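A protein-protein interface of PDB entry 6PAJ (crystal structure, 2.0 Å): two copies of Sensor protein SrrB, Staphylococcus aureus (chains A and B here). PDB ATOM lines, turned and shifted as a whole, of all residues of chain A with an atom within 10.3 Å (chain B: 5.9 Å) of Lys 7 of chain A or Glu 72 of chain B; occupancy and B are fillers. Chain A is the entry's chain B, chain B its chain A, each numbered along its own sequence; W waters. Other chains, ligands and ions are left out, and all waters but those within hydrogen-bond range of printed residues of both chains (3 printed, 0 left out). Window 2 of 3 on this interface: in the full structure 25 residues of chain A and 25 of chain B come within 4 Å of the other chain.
Among the printed residues, pairs that only touch across the chains: Ile 10 of chain A with Ala 67 of chain B (3.6 Å), Ile 10 of chain A with Arg 68 of chain B (3.6 Å), Lys 7 of chain A with Glu 72 of chain B (3.7 Å), Ile 10 of chain A with Ala 71 of chain B (3.7 Å) and Lys 7 of chain A with Ala 71 of chain B (3.97 Å).
Of chain B, only Ala 71 (3.97 Å) and Glu 72 (3.7 Å) come within 4 Å of Lys 7 of chain A.
Printed residues of chain B within 4 Å of Ile 10 of chain A: Ala 67 (3.6 Å), Arg 68 (3.6 Å) and Ala 71 (3.7 Å).
Val 13 of chain A touches none of the printed residues of chain B.
Printed residues of chain B within 4 Å of Ser 14 of chain A: Arg 68 (2.9 Å).
Of the printed residues of chain A, Ala 67 of chain B touches Ile 10 (3.6 Å).
Of the printed residues of chain A, Arg 68 of chain B touches Ile 10 and Ser 14.
Of chain A, only Lys 7 and Ile 10 come within 4 Å of Ala 71 of chain B.
Printed residues of chain A within 4 Å of Glu 72 of chain B: Lys 7.
No residue of chain A comes within 4 Å of Gly 73 of chain B.
No residue of chain A comes within 4 Å of Ser 75 of chain B.
The nearest residue of chain A that does not touch Glu 72 of chain B is Asp 3 of chain A (6.1 Å).
1 position is printed for both chains.
Of the 6 pairs that touch across the chains among the printed residues, none has its exchanged pair printed and touching as well.
Water W1 bridges the backbone carbonyl oxygen of Ala 71 of chain B (2.5 Å) and the side-chain carboxylate of Asp 3 of chain A (2.6 Å).
Water W2 lies within hydrogen-bond range of the side-chain amino group (NZ) of Lys 7 of chain A (2.6 Å), the backbone carbonyl oxygen (O) of Ala 71 of chain B (3.0 Å) and the side-chain carboxylate (OD2) of Asp 3 of chain A (3.5 Å).
Water W3 lies within hydrogen-bond range of the side-chain amino group of Lys 7 of chain A, the backbone carbonyl oxygen of Glu 72 of chain B and the side-chain hydroxyl of Ser 75 of chain B.
Of the 21 printed residues of chain A, 3 touch a printed residue of chain B.
Hydrophobic or aromatic side chains of chain A that line the printed part of chain B: Ile 10.
Hydrophobic or aromatic side chains of chain B that line the printed part of chain A: Ala 67 and Ala 71.
Along chain B the printed residues that touch a printed residue of chain A span positions 67 to 72.
The guanidinium group of Arg 68 of chain B lies within hydrogen-bond range of the side-chain hydroxyl of Ser 14 of chain A, at 2.9 Å.
OE1 of Gln 124 of chain B sits close to OE1 of Glu 72 of chain B, at 3.0 Å.
The side-chain hydroxyl of Ser 75 of chain B lies close to the backbone carbonyl oxygen of Glu 72 of chain B (3.3 Å).
The backbone carbonyl oxygen (O) of Ile 10 of chain A lies within hydrogen-bond range of the side-chain hydroxyl (OG) of Ser 14 of chain A, at 2.7 Å.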
ATOM      1  N   ASN A   1      -8.204 -12.525  18.274  1.00  0.00           N
ATOM      2  CA  ASN A   1      -7.283 -11.951  19.301  1.00  0.00           C
ATOM      3  C   ASN A   1      -6.041 -12.837  19.467  1.00  0.00           C
ATOM      4  O   ASN A   1      -5.275 -12.666  20.406  1.00  0.00           O
ATOM      5  CB  ASN A   1      -7.997 -11.713  20.630  1.00  0.00           C
ATOM      6  CG  ASN A   1      -8.125 -10.235  20.930  1.00  0.00           C
ATOM      7  OD1 ASN A   1      -7.162  -9.484  20.766  1.00  0.00           O
ATOM      8  ND2 ASN A   1      -9.306  -9.813  21.356  1.00  0.00           N
ATOM      9  N   LEU A   2      -5.815 -13.731  18.515  1.00  0.00           N
ATOM     10  CA  LEU A   2      -4.617 -14.526  18.487  1.00  0.00           C
ATOM     11  C   LEU A   2      -3.410 -13.587  18.333  1.00  0.00           C
ATOM     12  O   LEU A   2      -2.401 -13.764  19.014  1.00  0.00           O
ATOM     13  CB  LEU A   2      -4.725 -15.535  17.338  1.00  0.00           C
ATOM     14  CG  LEU A   2      -3.828 -16.769  17.410  1.00  0.00           C
ATOM     15  CD1 LEU A   2      -3.542 -17.205  18.841  1.00  0.00           C
ATOM     16  CD2 LEU A   2      -4.450 -17.919  16.630  1.00  0.00           C
ATOM     17  N   ASP A   3      -3.528 -12.574  17.469  1.00  0.00           N
ATOM     18  CA  ASP A   3      -2.424 -11.644  17.204  1.00  0.00           C
ATOM     19  C   ASP A   3      -1.938 -10.996  18.507  1.00  0.00           C
ATOM     20  O   ASP A   3      -0.727 -10.884  18.707  1.00  0.00           O
ATOM     21  CB  ASP A   3      -2.810 -10.530  16.227  1.00  0.00           C
ATOM     22  CG  ASP A   3      -2.833 -10.959  14.775  1.00  0.00           C
ATOM     23  OD1 ASP A   3      -2.182 -11.970  14.445  1.00  0.00           O
ATOM     24  OD2 ASP A   3      -3.507 -10.262  13.984  1.00  0.00           O
ATOM     25  N   GLN A   4      -2.857 -10.543  19.362  1.00  0.00           N
ATOM     26  CA  GLN A   4      -2.445  -9.853  20.582  1.00  0.00           C
ATOM     27  C   GLN A   4      -1.757 -10.836  21.540  1.00  0.00           C
ATOM     28  O   GLN A   4      -0.787 -10.461  22.202  1.00  0.00           O
ATOM     29  CB  GLN A   4      -3.619  -9.157  21.283  1.00  0.00           C
ATOM     30  CG  GLN A   4      -3.159  -8.177  22.368  1.00  0.00           C
ATOM     31  CD  GLN A   4      -2.271  -7.047  21.877  1.00  0.00           C
ATOM     32  OE1 GLN A   4      -2.685  -6.195  21.095  1.00  0.00           O
ATOM     33  NE2 GLN A   4      -1.030  -7.013  22.342  1.00  0.00           N
ATOM     34  N   MET A   5      -2.288 -12.059  21.626  1.00  0.00           N
ATOM     35  CA  MET A   5      -1.713 -13.134  22.424  1.00  0.00           C
ATOM     36  C   MET A   5      -0.249 -13.356  22.023  1.00  0.00           C
ATOM     37  O   MET A   5       0.579 -13.547  22.890  1.00  0.00           O
ATOM     38  CB  MET A   5      -2.469 -14.456  22.227  1.00  0.00           C
ATOM     39  CG  MET A   5      -3.412 -14.838  23.355  1.00  0.00           C
ATOM     40  SD  MET A   5      -4.053 -16.566  23.187  1.00  0.00           S
ATOM     41  CE  MET A   5      -5.265 -16.368  21.884  1.00  0.00           C
ATOM     42  N   LYS A   6       0.018 -13.375  20.714  1.00  0.00           N
ATOM     43  CA  LYS A   6       1.354 -13.604  20.159  1.00  0.00           C
ATOM     44  C   LYS A   6       2.274 -12.447  20.556  1.00  0.00           C
ATOM     45  O   LYS A   6       3.407 -12.664  21.012  1.00  0.00           O
ATOM     46  CB  LYS A   6       1.294 -13.821  18.645  1.00  0.00           C
ATOM     47  CG  LYS A   6       0.748 -15.178  18.236  1.00  0.00           C
ATOM     48  CD  LYS A   6       0.790 -15.453  16.747  1.00  0.00           C
ATOM     49  CE  LYS A   6       0.332 -16.863  16.439  1.00  0.00           C
ATOM     50  NZ  LYS A   6      -0.174 -16.995  15.054  1.00  0.00           N
ATOM     51  N   LYS A   7       1.779 -11.228  20.428  1.00  0.00           N
ATOM     52  CA  LYS A   7       2.541 -10.042  20.856  1.00  0.00           C
ATOM     53  C   LYS A   7       2.886 -10.107  22.344  1.00  0.00           C
ATOM     54  O   LYS A   7       4.021  -9.901  22.750  1.00  0.00           O
ATOM     55  CB  LYS A   7       1.751  -8.759  20.565  1.00  0.00           C
ATOM     56  CG  LYS A   7       1.712  -8.379  19.087  1.00  0.00           C
ATOM     57  CD  LYS A   7       0.753  -7.237  18.775  1.00  0.00           C
ATOM     58  CE  LYS A   7       0.432  -7.108  17.301  1.00  0.00           C
ATOM     59  NZ  LYS A   7      -1.011  -6.871  17.066  1.00  0.00           N
ATOM     60  N   ASP A   8       1.901 -10.382  23.171  1.00  0.00           N
ATOM     61  CA  ASP A   8       2.144 -10.432  24.597  1.00  0.00           C
ATOM     62  C   ASP A   8       3.084 -11.606  24.915  1.00  0.00           C
ATOM     63  O   ASP A   8       3.891 -11.500  25.792  1.00  0.00           O
ATOM     64  CB  ASP A   8       0.832 -10.528  25.383  1.00  0.00           C
ATOM     65  CG  ASP A   8      -0.121  -9.350  25.203  1.00  0.00           C
ATOM     66  OD1 ASP A   8       0.368  -8.225  24.906  1.00  0.00           O
ATOM     67  OD2 ASP A   8      -1.347  -9.559  25.387  1.00  0.00           O
ATOM     68  N   PHE A   9       2.976 -12.731  24.212  1.00  0.00           N
ATOM     69  CA  PHE A   9       3.895 -13.868  24.443  1.00  0.00           C
ATOM     70  C   PHE A   9       5.322 -13.417  24.112  1.00  0.00           C
ATOM     71  O   PHE A   9       6.239 -13.648  24.856  1.00  0.00           O
ATOM     72  CB  PHE A   9       3.466 -15.068  23.595  1.00  0.00           C
ATOM     73  CG  PHE A   9       4.418 -16.240  23.603  1.00  0.00           C
ATOM     74  CD1 PHE A   9       4.325 -17.220  24.572  1.00  0.00           C
ATOM     75  CD2 PHE A   9       5.396 -16.374  22.634  1.00  0.00           C
ATOM     76  CE1 PHE A   9       5.202 -18.297  24.585  1.00  0.00           C
ATOM     77  CE2 PHE A   9       6.253 -17.455  22.620  1.00  0.00           C
ATOM     78  CZ  PHE A   9       6.155 -18.417  23.598  1.00  0.00           C
ATOM     79  N   ILE A  10       5.521 -12.748  22.983  1.00  0.00           N
ATOM     80  CA  ILE A  10       6.878 -12.397  22.581  1.00  0.00           C
ATOM     81  C   ILE A  10       7.461 -11.415  23.599  1.00  0.00           C
ATOM     82  O   ILE A  10       8.641 -11.558  24.005  1.00  0.00           O
ATOM     83  CB  ILE A  10       6.908 -11.852  21.139  1.00  0.00           C
ATOM     84  CG1 ILE A  10       6.554 -12.961  20.151  1.00  0.00           C
ATOM     85  CG2 ILE A  10       8.248 -11.199  20.802  1.00  0.00           C
ATOM     86  CD1 ILE A  10       6.149 -12.479  18.795  1.00  0.00           C
ATOM     87  N   ALA A  11       6.628 -10.468  24.052  1.00  0.00           N
ATOM     88  CA  ALA A  11       7.053  -9.483  25.030  1.00  0.00           C
ATOM     89  C   ALA A  11       7.506 -10.181  26.325  1.00  0.00           C
ATOM     90  O   ALA A  11       8.539  -9.870  26.923  1.00  0.00           O
ATOM     91  CB  ALA A  11       5.916  -8.512  25.288  1.00  0.00           C
ATOM     92  N   ASN A  12       6.719 -11.143  26.773  1.00  0.00           N
ATOM     93  CA  ASN A  12       7.009 -11.815  28.020  1.00  0.00           C
ATOM     94  C   ASN A  12       8.300 -12.633  27.871  1.00  0.00           C
ATOM     95  O   ASN A  12       9.187 -12.614  28.732  1.00  0.00           O
ATOM     96  CB  ASN A  12       5.808 -12.663  28.457  1.00  0.00           C
ATOM     97  CG  ASN A  12       6.100 -13.410  29.734  1.00  0.00           C
ATOM     98  OD1 ASN A  12       6.289 -12.791  30.779  1.00  0.00           O
ATOM     99  ND2 ASN A  12       6.166 -14.726  29.659  1.00  0.00           N
ATOM    100  N   VAL A  13       8.389 -13.376  26.778  1.00  0.00           N
ATOM    101  CA  VAL A  13       9.574 -14.199  26.454  1.00  0.00           C
ATOM    102  C   VAL A  13      10.867 -13.366  26.421  1.00  0.00           C
ATOM    103  O   VAL A  13      11.923 -13.804  26.961  1.00  0.00           O
ATOM    104  CB  VAL A  13       9.352 -14.943  25.125  1.00  0.00           C
ATOM    105  CG1 VAL A  13      10.632 -15.192  24.355  1.00  0.00           C
ATOM    106  CG2 VAL A  13       8.615 -16.241  25.361  1.00  0.00           C
ATOM    107  N   SER A  14      10.835 -12.206  25.774  1.00  0.00           N
ATOM    108  CA  SER A  14      12.031 -11.336  25.739  1.00  0.00           C
ATOM    109  C   SER A  14      12.574 -11.077  27.140  1.00  0.00           C
ATOM    110  O   SER A  14      13.791 -11.181  27.335  1.00  0.00           O
ATOM    111  CB  SER A  14      11.796  -9.976  25.064  1.00  0.00           C
ATOM    112  OG  SER A  14      10.960 -10.086  23.931  1.00  0.00           O
ATOM    113  N   HIS A  15      11.696 -10.681  28.068  1.00  0.00           N
ATOM    114  CA  HIS A  15      12.105 -10.415  29.425  1.00  0.00           C
ATOM    115  C   HIS A  15      12.666 -11.687  30.085  1.00  0.00           C
ATOM    116  O   HIS A  15      13.713 -11.658  30.709  1.00  0.00           O
ATOM    117  CB  HIS A  15      10.953  -9.822  30.248  1.00  0.00           C
ATOM    118  CG  HIS A  15      11.372  -9.417  31.626  1.00  0.00           C
ATOM    119  ND1 HIS A  15      11.279 -10.276  32.719  1.00  0.00           N
ATOM    120  CD2 HIS A  15      11.945  -8.277  32.084  1.00  0.00           C
ATOM    121  CE1 HIS A  15      11.749  -9.664  33.790  1.00  0.00           C
ATOM    122  NE2 HIS A  15      12.167  -8.437  33.424  1.00  0.00           N
ATOM    123  N   ASP A  70       3.413 -23.672  16.456  1.00  0.00           N
ATOM    124  CA  ASP A  70       2.806 -22.612  15.683  1.00  0.00           C
ATOM    125  C   ASP A  70       3.108 -22.778  14.180  1.00  0.00           C
ATOM    126  O   ASP A  70       2.204 -22.701  13.374  1.00  0.00           O
ATOM    127  CB  ASP A  70       3.298 -21.243  16.158  1.00  0.00           C
ATOM    128  CG  ASP A  70       2.421 -20.101  15.681  1.00  0.00           C
ATOM    129  OD1 ASP A  70       1.209 -20.323  15.519  1.00  0.00           O
ATOM    130  OD2 ASP A  70       2.953 -19.001  15.513  1.00  0.00           O
ATOM    131  N   GLN A 189      -2.122 -12.450  30.268  1.00  0.00           N
ATOM    132  CA  GLN A 189      -1.397 -11.929  29.112  1.00  0.00           C
ATOM    133  C   GLN A 189       0.048 -12.459  29.092  1.00  0.00           C
ATOM    134  O   GLN A 189       0.770 -12.239  28.114  1.00  0.00           O
ATOM    135  CB  GLN A 189      -1.433 -10.420  29.129  1.00  0.00           C
ATOM    136  N   GLY A 190       0.465 -13.186  30.135  1.00  0.00           N
ATOM    137  CA  GLY A 190       1.860 -13.659  30.255  1.00  0.00           C
ATOM    138  C   GLY A 190       1.951 -15.170  30.434  1.00  0.00           C
ATOM    139  O   GLY A 190       2.509 -15.656  31.420  1.00  0.00           O
ATOM    140  N   THR A 191       1.411 -15.935  29.495  1.00  0.00           N
ATOM    141  CA  THR A 191       0.720 -15.412  28.308  1.00  0.00           C
ATOM    142  C   THR A 191      -0.520 -16.264  28.016  1.00  0.00           C
ATOM    143  O   THR A 191      -1.621 -15.731  27.776  1.00  0.00           O
ATOM    144  CB  THR A 191       1.646 -15.376  27.089  1.00  0.00           C
ATOM    145  OG1 THR A 191       0.871 -15.594  25.904  1.00  0.00           O
ATOM    146  CG2 THR A 191       2.746 -16.405  27.193  1.00  0.00           C
ATOM    147  N   GLY A 192      -0.318 -17.576  28.020  1.00  0.00           N
ATOM    148  CA  GLY A 192      -1.353 -18.494  27.669  1.00  0.00           C
ATOM    149  C   GLY A 192      -1.207 -19.005  26.244  1.00  0.00           C
ATOM    150  O   GLY A 192      -1.944 -19.908  25.865  1.00  0.00           O
ATOM    151  N   LEU A 193      -0.275 -18.457  25.450  1.00  0.00           N
ATOM    152  CA  LEU A 193      -0.223 -18.795  24.050  1.00  0.00           C
ATOM    153  C   LEU A 193       0.047 -20.300  23.904  1.00  0.00           C
ATOM    154  O   LEU A 193      -0.637 -20.960  23.137  1.00  0.00           O
ATOM    155  CB  LEU A 193       0.862 -17.998  23.316  1.00  0.00           C
ATOM    156  CG  LEU A 193       1.003 -18.317  21.825  1.00  0.00           C
ATOM    157  CD1 LEU A 193      -0.302 -18.078  21.073  1.00  0.00           C
ATOM    158  CD2 LEU A 193       2.118 -17.518  21.186  1.00  0.00           C
ATOM    159  N   ALA B  67      10.428 -12.425  15.239  1.00  0.00           N
ATOM    160  CA  ALA B  67       9.127 -12.923  15.738  1.00  0.00           C
ATOM    161  C   ALA B  67       8.126 -11.752  15.827  1.00  0.00           C
ATOM    162  O   ALA B  67       6.978 -11.884  15.389  1.00  0.00           O
ATOM    163  CB  ALA B  67       9.296 -13.617  17.077  1.00  0.00           C
ATOM    164  N   ARG B  68       8.565 -10.622  16.383  1.00  0.00           N
ATOM    165  CA  ARG B  68       7.705  -9.446  16.495  1.00  0.00           C
ATOM    166  C   ARG B  68       7.213  -9.012  15.110  1.00  0.00           C
ATOM    167  O   ARG B  68       6.042  -8.683  14.950  1.00  0.00           O
ATOM    168  CB  ARG B  68       8.438  -8.261  17.112  1.00  0.00           C
ATOM    169  CG  ARG B  68       8.654  -8.378  18.608  1.00  0.00           C
ATOM    170  CD  ARG B  68       9.581  -7.281  19.085  1.00  0.00           C
ATOM    171  NE  ARG B  68      10.028  -7.530  20.449  1.00  0.00           N
ATOM    172  CZ  ARG B  68      11.295  -7.575  20.846  1.00  0.00           C
ATOM    173  NH1 ARG B  68      12.282  -7.295  19.999  1.00  0.00           N
ATOM    174  NH2 ARG B  68      11.557  -7.888  22.108  1.00  0.00           N
ATOM    175  N   MET B  69       8.114  -9.034  14.130  1.00  0.00           N
ATOM    176  CA  MET B  69       7.819  -8.644  12.774  1.00  0.00           C
ATOM    177  C   MET B  69       6.751  -9.556  12.171  1.00  0.00           C
ATOM    178  O   MET B  69       5.894  -9.056  11.442  1.00  0.00           O
ATOM    179  CB  MET B  69       9.062  -8.713  11.875  1.00  0.00           C
ATOM    180  CG  MET B  69       9.831  -7.415  11.855  1.00  0.00           C
ATOM    181  SD  MET B  69      10.858  -7.227  10.358  1.00  0.00           S
ATOM    182  CE  MET B  69      11.903  -8.655  10.595  1.00  0.00           C
ATOM    183  N   ASP B  70       6.847 -10.868  12.412  1.00  0.00           N
ATOM    184  CA  ASP B  70       5.868 -11.817  11.882  1.00  0.00           C
ATOM    185  C   ASP B  70       4.520 -11.626  12.591  1.00  0.00           C
ATOM    186  O   ASP B  70       3.463 -11.807  11.967  1.00  0.00           O
ATOM    187  CB  ASP B  70       6.339 -13.261  12.045  1.00  0.00           C
ATOM    188  CG  ASP B  70       5.441 -14.296  11.373  1.00  0.00           C
ATOM    189  OD1 ASP B  70       4.930 -14.025  10.269  1.00  0.00           O
ATOM    190  OD2 ASP B  70       5.280 -15.378  11.954  1.00  0.00           O
ATOM    191  N   ALA B  71       4.567 -11.269  13.875  1.00  0.00           N
ATOM    192  CA  ALA B  71       3.374 -11.210  14.741  1.00  0.00           C
ATOM    193  C   ALA B  71       2.513  -9.968  14.437  1.00  0.00           C
ATOM    194  O   ALA B  71       1.315  -9.970  14.696  1.00  0.00           O
ATOM    195  CB  ALA B  71       3.798 -11.228  16.186  1.00  0.00           C
ATOM    196  N   GLU B  72       3.108  -8.900  13.914  1.00  0.00           N
ATOM    197  CA  GLU B  72       2.353  -7.676  13.572  1.00  0.00           C
ATOM    198  C   GLU B  72       1.816  -7.772  12.131  1.00  0.00           C
ATOM    199  O   GLU B  72       1.114  -6.875  11.662  1.00  0.00           O
ATOM    200  CB  GLU B  72       3.248  -6.451  13.763  1.00  0.00           C
ATOM    201  CG  GLU B  72       3.049  -5.744  15.087  1.00  0.00           C
ATOM    202  CD  GLU B  72       4.319  -5.447  15.863  1.00  0.00           C
ATOM    203  OE1 GLU B  72       4.752  -4.274  15.852  1.00  0.00           O
ATOM    204  OE2 GLU B  72       4.858  -6.384  16.496  1.00  0.00           O
ATOM    205  N   GLY B  73       2.153  -8.843  11.424  1.00  0.00           N
ATOM    206  CA  GLY B  73       1.746  -9.048  10.051  1.00  0.00           C
ATOM    207  C   GLY B  73       2.052  -7.846   9.163  1.00  0.00           C
ATOM    208  O   GLY B  73       3.156  -7.255   9.208  1.00  0.00           O
ATOM    209  N   LEU B  74       1.047  -7.472   8.371  1.00  0.00           N
ATOM    210  CA  LEU B  74       1.143  -6.375   7.407  1.00  0.00           C
ATOM    211  C   LEU B  74       0.641  -5.062   8.023  1.00  0.00           C
ATOM    212  O   LEU B  74       0.367  -4.144   7.280  1.00  0.00           O
ATOM    213  CB  LEU B  74       0.304  -6.728   6.174  1.00  0.00           C
ATOM    214  CG  LEU B  74       0.525  -8.131   5.612  1.00  0.00           C
ATOM    215  CD1 LEU B  74      -0.759  -8.683   5.007  1.00  0.00           C
ATOM    216  CD2 LEU B  74       1.660  -8.139   4.598  1.00  0.00           C
ATOM    217  N   SER B  75       0.530  -4.949   9.346  1.00  0.00           N
ATOM    218  CA  SER B  75      -0.013  -3.712   9.958  1.00  0.00           C
ATOM    219  C   SER B  75       0.973  -2.542   9.786  1.00  0.00           C
ATOM    220  O   SER B  75       2.055  -2.557  10.390  1.00  0.00           O
ATOM    221  CB  SER B  75      -0.365  -3.915  11.424  1.00  0.00           C
ATOM    222  OG  SER B  75      -1.485  -4.779  11.564  1.00  0.00           O
ATOM    223  N   ASP B 120       7.657   1.776  14.237  1.00  0.00           N
ATOM    224  CA  ASP B 120       7.912   0.513  14.896  1.00  0.00           C
ATOM    225  C   ASP B 120       8.135  -0.548  13.828  1.00  0.00           C
ATOM    226  O   ASP B 120       8.947  -1.405  14.040  1.00  0.00           O
ATOM    227  CB  ASP B 120       6.812   0.136  15.897  1.00  0.00           C
ATOM    228  CG  ASP B 120       6.880   0.902  17.216  1.00  0.00           C
ATOM    229  OD1 ASP B 120       7.950   1.462  17.548  1.00  0.00           O
ATOM    230  OD2 ASP B 120       5.860   0.935  17.908  1.00  0.00           O
ATOM    231  N   ARG B 121       7.467  -0.460  12.678  1.00  0.00           N
ATOM    232  CA  ARG B 121       7.712  -1.426  11.662  1.00  0.00           C
ATOM    233  C   ARG B 121       9.086  -1.130  11.025  1.00  0.00           C
ATOM    234  O   ARG B 121       9.809  -2.084  10.692  1.00  0.00           O
ATOM    235  CB  ARG B 121       6.573  -1.495  10.636  1.00  0.00           C
ATOM    236  CG  ARG B 121       5.179  -1.769  11.195  1.00  0.00           C
ATOM    237  CD  ARG B 121       5.004  -2.979  12.106  1.00  0.00           C
ATOM    238  NE  ARG B 121       5.572  -4.241  11.636  1.00  0.00           N
ATOM    239  CZ  ARG B 121       4.916  -5.177  10.953  1.00  0.00           C
ATOM    240  NH1 ARG B 121       3.742  -4.915  10.403  1.00  0.00           N
ATOM    241  NH2 ARG B 121       5.456  -6.370  10.785  1.00  0.00           N
ATOM    242  N   GLN B 124      11.867  -2.387  13.252  1.00  0.00           N
ATOM    243  CA  GLN B 124      11.989  -3.817  13.060  1.00  0.00           C
ATOM    244  C   GLN B 124      12.810  -4.137  11.809  1.00  0.00           C
ATOM    245  O   GLN B 124      13.703  -5.021  11.871  1.00  0.00           O
ATOM    246  CB  GLN B 124      10.604  -4.471  12.962  1.00  0.00           C
ATOM    247  CG  GLN B 124       9.898  -4.581  14.306  1.00  0.00           C
ATOM    248  CD  GLN B 124       8.407  -4.774  14.164  1.00  0.00           C
ATOM    249  OE1 GLN B 124       7.646  -4.503  15.090  1.00  0.00           O
ATOM    250  NE2 GLN B 124       7.965  -5.190  12.989  1.00  0.00           N
HETATM  251  O   HOH W   1       0.318 -12.292  14.907  1.00  0.00           O
HETATM  252  O   HOH W   2      -0.943  -8.043  14.729  1.00  0.00           O
HETATM  253  O   HOH W   3       0.111  -5.364  14.571  1.00  0.00           O
